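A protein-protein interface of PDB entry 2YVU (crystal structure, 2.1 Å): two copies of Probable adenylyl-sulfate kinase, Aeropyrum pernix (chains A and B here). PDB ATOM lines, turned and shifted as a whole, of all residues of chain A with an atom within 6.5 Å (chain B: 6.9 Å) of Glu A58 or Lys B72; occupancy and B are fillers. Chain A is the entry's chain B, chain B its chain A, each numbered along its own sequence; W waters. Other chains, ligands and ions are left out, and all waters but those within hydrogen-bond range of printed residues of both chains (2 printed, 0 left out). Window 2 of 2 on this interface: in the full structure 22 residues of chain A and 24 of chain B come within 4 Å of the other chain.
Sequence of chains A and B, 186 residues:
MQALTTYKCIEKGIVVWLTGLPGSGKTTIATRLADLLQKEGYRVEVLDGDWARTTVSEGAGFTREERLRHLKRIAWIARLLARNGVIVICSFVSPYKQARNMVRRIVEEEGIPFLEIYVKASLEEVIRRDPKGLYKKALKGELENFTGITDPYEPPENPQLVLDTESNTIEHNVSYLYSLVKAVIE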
ATOM      1  N   ALA A  52     -10.018 -21.151 -23.253  1.00  0.00           N
ATOM      2  CA  ALA A  52      -9.367 -20.661 -22.044  1.00  0.00           C
ATOM      3  C   ALA A  52      -9.698 -21.424 -20.755  1.00  0.00           C
ATOM      4  O   ALA A  52      -8.798 -21.759 -19.957  1.00  0.00           O
ATOM      5  CB  ALA A  52      -9.697 -19.191 -21.873  1.00  0.00           C
ATOM      6  N   ARG A  53     -10.988 -21.686 -20.540  1.00  0.00           N
ATOM      7  CA  ARG A  53     -11.442 -22.393 -19.343  1.00  0.00           C
ATOM      8  C   ARG A  53     -10.691 -23.697 -19.056  1.00  0.00           C
ATOM      9  O   ARG A  53     -10.486 -24.062 -17.903  1.00  0.00           O
ATOM     10  CB  ARG A  53     -12.947 -22.689 -19.444  1.00  0.00           C
ATOM     11  CG  ARG A  53     -13.838 -21.626 -18.830  1.00  0.00           C
ATOM     12  CD  ARG A  53     -15.290 -22.103 -18.775  1.00  0.00           C
ATOM     13  NE  ARG A  53     -15.888 -22.183 -20.107  1.00  0.00           N
ATOM     14  CZ  ARG A  53     -16.296 -21.129 -20.806  1.00  0.00           C
ATOM     15  NH1 ARG A  53     -16.180 -19.899 -20.303  1.00  0.00           N
ATOM     16  NH2 ARG A  53     -16.815 -21.299 -22.017  1.00  0.00           N
ATOM     17  N   THR A  54     -10.279 -24.394 -20.099  1.00  0.00           N
ATOM     18  CA  THR A  54      -9.572 -25.650 -19.931  1.00  0.00           C
ATOM     19  C   THR A  54      -8.045 -25.521 -20.046  1.00  0.00           C
ATOM     20  O   THR A  54      -7.321 -26.468 -19.740  1.00  0.00           O
ATOM     21  CB  THR A  54     -10.036 -26.666 -20.993  1.00  0.00           C
ATOM     22  OG1 THR A  54      -9.356 -27.913 -20.804  1.00  0.00           O
ATOM     23  CG2 THR A  54      -9.721 -26.154 -22.372  1.00  0.00           C
ATOM     24  N   THR A  55      -7.552 -24.358 -20.464  1.00  0.00           N
ATOM     25  CA  THR A  55      -6.118 -24.198 -20.652  1.00  0.00           C
ATOM     26  C   THR A  55      -5.398 -23.136 -19.817  1.00  0.00           C
ATOM     27  O   THR A  55      -4.830 -23.448 -18.771  1.00  0.00           O
ATOM     28  CB  THR A  55      -5.810 -23.940 -22.147  1.00  0.00           C
ATOM     29  OG1 THR A  55      -6.448 -22.735 -22.571  1.00  0.00           O
ATOM     30  CG2 THR A  55      -6.336 -25.078 -23.000  1.00  0.00           C
ATOM     31  N   VAL A  56      -5.432 -21.886 -20.269  1.00  0.00           N
ATOM     32  CA  VAL A  56      -4.721 -20.826 -19.568  1.00  0.00           C
ATOM     33  C   VAL A  56      -5.507 -20.187 -18.450  1.00  0.00           C
ATOM     34  O   VAL A  56      -4.941 -19.587 -17.540  1.00  0.00           O
ATOM     35  CB  VAL A  56      -4.243 -19.718 -20.547  1.00  0.00           C
ATOM     36  CG1 VAL A  56      -3.456 -20.353 -21.671  1.00  0.00           C
ATOM     37  CG2 VAL A  56      -5.436 -18.911 -21.086  1.00  0.00           C
ATOM     38  N   SER A  57      -6.821 -20.322 -18.493  1.00  0.00           N
ATOM     39  CA  SER A  57      -7.609 -19.721 -17.443  1.00  0.00           C
ATOM     40  C   SER A  57      -8.360 -20.732 -16.626  1.00  0.00           C
ATOM     41  O   SER A  57      -9.322 -20.397 -15.948  1.00  0.00           O
ATOM     42  CB  SER A  57      -8.561 -18.687 -18.023  1.00  0.00           C
ATOM     43  OG  SER A  57      -7.808 -17.564 -18.423  1.00  0.00           O
ATOM     44  N   GLU A  58      -7.907 -21.974 -16.677  1.00  0.00           N
ATOM     45  CA  GLU A  58      -8.547 -23.015 -15.903  1.00  0.00           C
ATOM     46  C   GLU A  58      -8.383 -22.710 -14.415  1.00  0.00           C
ATOM     47  O   GLU A  58      -7.271 -22.472 -13.928  1.00  0.00           O
ATOM     48  CB  GLU A  58      -7.927 -24.360 -16.235  1.00  0.00           C
ATOM     49  CG  GLU A  58      -8.479 -25.508 -15.424  1.00  0.00           C
ATOM     50  CD  GLU A  58      -8.038 -26.848 -15.974  1.00  0.00           C
ATOM     51  OE1 GLU A  58      -8.869 -27.534 -16.616  1.00  0.00           O
ATOM     52  OE2 GLU A  58      -6.857 -27.210 -15.774  1.00  0.00           O
ATOM     53  N   GLY A  59      -9.494 -22.696 -13.687  1.00  0.00           N
ATOM     54  CA  GLY A  59      -9.400 -22.412 -12.270  1.00  0.00           C
ATOM     55  C   GLY A  59     -10.437 -21.425 -11.795  1.00  0.00           C
ATOM     56  O   GLY A  59     -10.136 -20.501 -11.035  1.00  0.00           O
ATOM     57  N   ALA A  60     -11.666 -21.635 -12.254  1.00  0.00           N
ATOM     58  CA  ALA A  60     -12.808 -20.807 -11.894  1.00  0.00           C
ATOM     59  C   ALA A  60     -12.472 -19.340 -11.663  1.00  0.00           C
ATOM     60  O   ALA A  60     -11.490 -18.811 -12.188  1.00  0.00           O
ATOM     61  CB  ALA A  60     -13.495 -21.386 -10.654  1.00  0.00           C
ATOM     62  N   ARG A  73      -4.498 -11.526 -18.956  1.00  0.00           N
ATOM     63  CA  ARG A  73      -3.706 -12.666 -19.379  1.00  0.00           C
ATOM     64  C   ARG A  73      -3.925 -12.919 -20.883  1.00  0.00           C
ATOM     65  O   ARG A  73      -2.972 -13.158 -21.639  1.00  0.00           O
ATOM     66  CB  ARG A  73      -4.107 -13.904 -18.573  1.00  0.00           C
ATOM     67  CG  ARG A  73      -3.414 -15.144 -19.058  1.00  0.00           C
ATOM     68  CD  ARG A  73      -3.425 -16.247 -18.036  1.00  0.00           C
ATOM     69  NE  ARG A  73      -4.760 -16.579 -17.595  1.00  0.00           N
ATOM     70  CZ  ARG A  73      -5.182 -16.480 -16.338  1.00  0.00           C
ATOM     71  NH1 ARG A  73      -4.367 -16.056 -15.382  1.00  0.00           N
ATOM     72  NH2 ARG A  73      -6.433 -16.798 -16.050  1.00  0.00           N
ATOM     73  N   ARG B  67       0.994 -23.468  -8.419  1.00  0.00           N
ATOM     74  CA  ARG B  67       2.153 -23.509  -9.301  1.00  0.00           C
ATOM     75  C   ARG B  67       1.862 -24.353 -10.541  1.00  0.00           C
ATOM     76  O   ARG B  67       2.278 -24.007 -11.645  1.00  0.00           O
ATOM     77  CB  ARG B  67       3.364 -24.083  -8.558  1.00  0.00           C
ATOM     78  CG  ARG B  67       3.912 -23.171  -7.487  1.00  0.00           C
ATOM     79  CD  ARG B  67       5.091 -23.815  -6.757  1.00  0.00           C
ATOM     80  NE  ARG B  67       5.597 -22.962  -5.680  1.00  0.00           N
ATOM     81  CZ  ARG B  67       6.340 -21.871  -5.860  1.00  0.00           C
ATOM     82  NH1 ARG B  67       6.681 -21.484  -7.083  1.00  0.00           N
ATOM     83  NH2 ARG B  67       6.744 -21.163  -4.813  1.00  0.00           N
ATOM     84  N   LEU B  68       1.158 -25.463 -10.346  1.00  0.00           N
ATOM     85  CA  LEU B  68       0.797 -26.355 -11.442  1.00  0.00           C
ATOM     86  C   LEU B  68      -0.098 -25.639 -12.442  1.00  0.00           C
ATOM     87  O   LEU B  68       0.134 -25.703 -13.653  1.00  0.00           O
ATOM     88  CB  LEU B  68       0.052 -27.590 -10.921  1.00  0.00           C
ATOM     89  CG  LEU B  68       0.793 -28.923 -10.815  1.00  0.00           C
ATOM     90  CD1 LEU B  68      -0.197 -30.005 -10.380  1.00  0.00           C
ATOM     91  CD2 LEU B  68       1.422 -29.288 -12.158  1.00  0.00           C
ATOM     92  N   ARG B  69      -1.142 -24.987 -11.939  1.00  0.00           N
ATOM     93  CA  ARG B  69      -2.054 -24.256 -12.825  1.00  0.00           C
ATOM     94  C   ARG B  69      -1.241 -23.321 -13.703  1.00  0.00           C
ATOM     95  O   ARG B  69      -1.503 -23.157 -14.888  1.00  0.00           O
ATOM     96  CB  ARG B  69      -3.037 -23.406 -12.020  1.00  0.00           C
ATOM     97  CG  ARG B  69      -4.404 -24.013 -11.847  1.00  0.00           C
ATOM     98  CD  ARG B  69      -5.385 -22.999 -11.268  1.00  0.00           C
ATOM     99  NE  ARG B  69      -6.748 -23.516 -11.296  1.00  0.00           N
ATOM    100  CZ  ARG B  69      -7.163 -24.578 -10.615  1.00  0.00           C
ATOM    101  NH1 ARG B  69      -6.319 -25.247  -9.840  1.00  0.00           N
ATOM    102  NH2 ARG B  69      -8.424 -24.980 -10.710  1.00  0.00           N
ATOM    103  N   HIS B  70      -0.245 -22.709 -13.077  1.00  0.00           N
ATOM    104  CA  HIS B  70       0.639 -21.749 -13.722  1.00  0.00           C
ATOM    105  C   HIS B  70       1.476 -22.396 -14.809  1.00  0.00           C
ATOM    106  O   HIS B  70       1.524 -21.906 -15.936  1.00  0.00           O
ATOM    107  CB  HIS B  70       1.491 -21.121 -12.623  1.00  0.00           C
ATOM    108  CG  HIS B  70       2.770 -20.518 -13.089  1.00  0.00           C
ATOM    109  ND1 HIS B  70       2.821 -19.386 -13.873  1.00  0.00           N
ATOM    110  CD2 HIS B  70       4.053 -20.837 -12.802  1.00  0.00           C
ATOM    111  CE1 HIS B  70       4.081 -19.030 -14.043  1.00  0.00           C
ATOM    112  NE2 HIS B  70       4.849 -19.895 -13.403  1.00  0.00           N
ATOM    113  N   LEU B  71       2.111 -23.513 -14.474  1.00  0.00           N
ATOM    114  CA  LEU B  71       2.952 -24.231 -15.415  1.00  0.00           C
ATOM    115  C   LEU B  71       2.166 -24.778 -16.604  1.00  0.00           C
ATOM    116  O   LEU B  71       2.648 -24.771 -17.740  1.00  0.00           O
ATOM    117  CB  LEU B  71       3.692 -25.362 -14.688  1.00  0.00           C
ATOM    118  CG  LEU B  71       4.713 -24.843 -13.657  1.00  0.00           C
ATOM    119  CD1 LEU B  71       5.326 -26.010 -12.879  1.00  0.00           C
ATOM    120  CD2 LEU B  71       5.822 -24.045 -14.370  1.00  0.00           C
ATOM    121  N   LYS B  72       0.960 -25.266 -16.351  1.00  0.00           N
ATOM    122  CA  LYS B  72       0.134 -25.780 -17.433  1.00  0.00           C
ATOM    123  C   LYS B  72      -0.193 -24.596 -18.355  1.00  0.00           C
ATOM    124  O   LYS B  72      -0.244 -24.717 -19.571  1.00  0.00           O
ATOM    125  CB  LYS B  72      -1.159 -26.369 -16.870  1.00  0.00           C
ATOM    126  CG  LYS B  72      -2.180 -26.716 -17.947  1.00  0.00           C
ATOM    127  CD  LYS B  72      -3.425 -27.343 -17.341  1.00  0.00           C
ATOM    128  CE  LYS B  72      -4.362 -27.864 -18.432  1.00  0.00           C
ATOM    129  NZ  LYS B  72      -5.606 -28.477 -17.855  1.00  0.00           N
ATOM    130  N   ARG B  73      -0.421 -23.445 -17.748  1.00  0.00           N
ATOM    131  CA  ARG B  73      -0.735 -22.251 -18.495  1.00  0.00           C
ATOM    132  C   ARG B  73       0.443 -21.855 -19.369  1.00  0.00           C
ATOM    133  O   ARG B  73       0.270 -21.509 -20.535  1.00  0.00           O
ATOM    134  CB  ARG B  73      -1.073 -21.130 -17.528  1.00  0.00           C
ATOM    135  CG  ARG B  73      -1.346 -19.841 -18.202  1.00  0.00           C
ATOM    136  CD  ARG B  73      -2.228 -19.035 -17.308  1.00  0.00           C
ATOM    137  NE  ARG B  73      -1.514 -18.668 -16.120  1.00  0.00           N
ATOM    138  CZ  ARG B  73      -2.018 -18.724 -14.897  1.00  0.00           C
ATOM    139  NH1 ARG B  73      -3.263 -19.141 -14.680  1.00  0.00           N
ATOM    140  NH2 ARG B  73      -1.258 -18.354 -13.893  1.00  0.00           N
ATOM    141  N   ILE B  74       1.643 -21.904 -18.801  1.00  0.00           N
ATOM    142  CA  ILE B  74       2.840 -21.565 -19.560  1.00  0.00           C
ATOM    143  C   ILE B  74       3.011 -22.532 -20.722  1.00  0.00           C
ATOM    144  O   ILE B  74       3.373 -22.129 -21.817  1.00  0.00           O
ATOM    145  CB  ILE B  74       4.107 -21.624 -18.681  1.00  0.00           C
ATOM    146  CG1 ILE B  74       4.071 -20.489 -17.646  1.00  0.00           C
ATOM    147  CG2 ILE B  74       5.354 -21.508 -19.558  1.00  0.00           C
ATOM    148  CD1 ILE B  74       3.846 -19.104 -18.261  1.00  0.00           C
ATOM    149  N   ALA B  75       2.751 -23.816 -20.465  1.00  0.00           N
ATOM    150  CA  ALA B  75       2.872 -24.851 -21.485  1.00  0.00           C
ATOM    151  C   ALA B  75       1.949 -24.548 -22.684  1.00  0.00           C
ATOM    152  O   ALA B  75       2.283 -24.776 -23.838  1.00  0.00           O
ATOM    153  CB  ALA B  75       2.500 -26.197 -20.877  1.00  0.00           C
ATOM    154  N   TRP B  76       0.776 -24.028 -22.408  1.00  0.00           N
ATOM    155  CA  TRP B  76      -0.119 -23.734 -23.510  1.00  0.00           C
ATOM    156  C   TRP B  76       0.310 -22.535 -24.324  1.00  0.00           C
ATOM    157  O   TRP B  76       0.222 -22.561 -25.555  1.00  0.00           O
ATOM    158  CB  TRP B  76      -1.524 -23.557 -22.990  1.00  0.00           C
ATOM    159  CG  TRP B  76      -2.222 -24.875 -22.983  1.00  0.00           C
ATOM    160  CD1 TRP B  76      -2.398 -25.719 -21.924  1.00  0.00           C
ATOM    161  CD2 TRP B  76      -2.796 -25.525 -24.119  1.00  0.00           C
ATOM    162  NE1 TRP B  76      -3.052 -26.853 -22.332  1.00  0.00           N
ATOM    163  CE2 TRP B  76      -3.310 -26.759 -23.676  1.00  0.00           C
ATOM    164  CE3 TRP B  76      -2.923 -25.178 -25.473  1.00  0.00           C
ATOM    165  CZ2 TRP B  76      -3.951 -27.657 -24.541  1.00  0.00           C
ATOM    166  CZ3 TRP B  76      -3.563 -26.071 -26.336  1.00  0.00           C
ATOM    167  CH2 TRP B  76      -4.069 -27.296 -25.861  1.00  0.00           C
ATOM    168  N   ILE B  77       0.788 -21.497 -23.634  1.00  0.00           N
ATOM    169  CA  ILE B  77       1.253 -20.279 -24.285  1.00  0.00           C
ATOM    170  C   ILE B  77       2.455 -20.660 -25.145  1.00  0.00           C
ATOM    171  O   ILE B  77       2.594 -20.208 -26.276  1.00  0.00           O
ATOM    172  CB  ILE B  77       1.682 -19.228 -23.248  1.00  0.00           C
ATOM    173  CG1 ILE B  77       0.466 -18.807 -22.408  1.00  0.00           C
ATOM    174  CG2 ILE B  77       2.362 -18.055 -23.934  1.00  0.00           C
ATOM    175  CD1 ILE B  77       0.786 -17.861 -21.211  1.00  0.00           C
ATOM    176  N   ALA B  99       5.421 -32.282 -12.634  1.00  0.00           N
ATOM    177  CA  ALA B  99       4.985 -31.000 -13.166  1.00  0.00           C
ATOM    178  C   ALA B  99       5.632 -30.747 -14.522  1.00  0.00           C
ATOM    179  O   ALA B  99       4.967 -30.346 -15.467  1.00  0.00           O
ATOM    180  CB  ALA B  99       5.341 -29.885 -12.178  1.00  0.00           C
ATOM    181  N   MET B 102       4.170 -32.992 -17.234  1.00  0.00           N
ATOM    182  CA  MET B 102       2.869 -32.481 -17.656  1.00  0.00           C
ATOM    183  C   MET B 102       3.083 -31.339 -18.681  1.00  0.00           C
ATOM    184  O   MET B 102       2.359 -31.226 -19.671  1.00  0.00           O
ATOM    185  CB  MET B 102       2.119 -31.986 -16.418  1.00  0.00           C
ATOM    186  CG  MET B 102       0.800 -31.319 -16.692  1.00  0.00           C
ATOM    187  SD  MET B 102       1.004 -29.573 -17.065  1.00  0.00           S
ATOM    188  CE  MET B 102       1.202 -28.872 -15.396  1.00  0.00           C
ATOM    189  N   VAL B 103       4.093 -30.503 -18.454  1.00  0.00           N
ATOM    190  CA  VAL B 103       4.384 -29.415 -19.392  1.00  0.00           C
ATOM    191  C   VAL B 103       4.840 -30.035 -20.719  1.00  0.00           C
ATOM    192  O   VAL B 103       4.332 -29.679 -21.780  1.00  0.00           O
ATOM    193  CB  VAL B 103       5.488 -28.494 -18.861  1.00  0.00           C
ATOM    194  CG1 VAL B 103       5.933 -27.533 -19.960  1.00  0.00           C
ATOM    195  CG2 VAL B 103       4.969 -27.709 -17.659  1.00  0.00           C
ATOM    196  N   ILE B 106       1.946 -31.482 -22.900  1.00  0.00           N
ATOM    197  CA  ILE B 106       1.170 -30.479 -23.594  1.00  0.00           C
ATOM    198  C   ILE B 106       1.886 -30.031 -24.848  1.00  0.00           C
ATOM    199  O   ILE B 106       1.274 -29.944 -25.915  1.00  0.00           O
ATOM    200  CB  ILE B 106       0.887 -29.292 -22.668  1.00  0.00           C
ATOM    201  CG1 ILE B 106      -0.132 -29.739 -21.609  1.00  0.00           C
ATOM    202  CG2 ILE B 106       0.422 -28.084 -23.481  1.00  0.00           C
ATOM    203  CD1 ILE B 106      -0.305 -28.793 -20.425  1.00  0.00           C
HETATM  204  O   HOH W   1      -5.297 -21.618 -15.180  1.00  0.00           O
HETATM  205  O   HOH W   2      -3.873 -23.611 -16.129  1.00  0.00           O
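Among the printed residues, pairs that only touch across the chains: Thr A55 with Trp B76, Val A56 with Trp B76 and Gly A59 with Arg B69.
The backbone carbonyl oxygen (O) of Ala A52 sits at hydrogen-bond distance from the backbone NH (N) of Glu A58 (3.4 Å). The guanidinium group of Arg A73 is in hydrogen-bond range of the backbone carbonyl oxygen of Val A56, at 3.0 Å. The guanidinium group of Arg A73 sits at hydrogen-bond distance from the side-chain hydroxyl of Ser A57, at 2.8 Å.
Printed residues of chain B within 4 Å of Val A56: Arg B73 (2.8 Å) and Trp B76 (3.97 Å). Of the printed residues of chain B, Arg A73 touches Arg B73 (3.1 Å). His B70 touches none of the printed residues of chain A. Lys B72 touches two residues of chain A. Ile B74 touches none of the printed residues of chain A. Of the printed residues of chain A, Trp B76 touches Thr A55 and Val A56. The nearest residue of chain B that does not touch Glu A58 is Arg B73 (5.3 Å). The nearest residue of chain A that does not touch Lys B72 is Thr A55 (4.3 Å).
Printed residues of chain A that touch a printed residue of chain B: Thr A54, Thr A55, Val A56, Glu A58, Gly A59 and Arg A73. Hydrophobic or aromatic side chains of chain A within 4 Å of the printed part of chain B: Val A56. Of the 15 printed residues of chain B, 4 touch a printed residue of chain A. Hydrophobic or aromatic side chains of chain B within 4 Å of the printed part of chain A: Trp B76. Among the printed residues, 8 pairs touch across the chains.
O of Glu A58 sits at hydrogen-bond distance from NE of Arg B69 (2.9 Å). O of Thr A54 is in hydrogen-bond range of NZ of Lys B72 (3.2 Å). NZ of Lys B72 is in salt-bridge range of OE2 of Glu A58, at 2.7 Å. NH1 of Arg B73 sits close to O of Val A56. The guanidinium group of Arg B73 lies close to the guanidinium group of Arg A73 (3.4 Å).
Water W1 lies within hydrogen-bond range of O of Glu A58, O of Val A56 and NH1 of Arg B73. Water W2 lies within hydrogen-bond range of the backbone carbonyl oxygen of Arg B69 (2.7 Å) and the backbone carbonyl oxygen of Thr A55 (2.8 Å).
Arg A73 touches its own counterpart, Arg B73. Position printed for both chains: 73.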
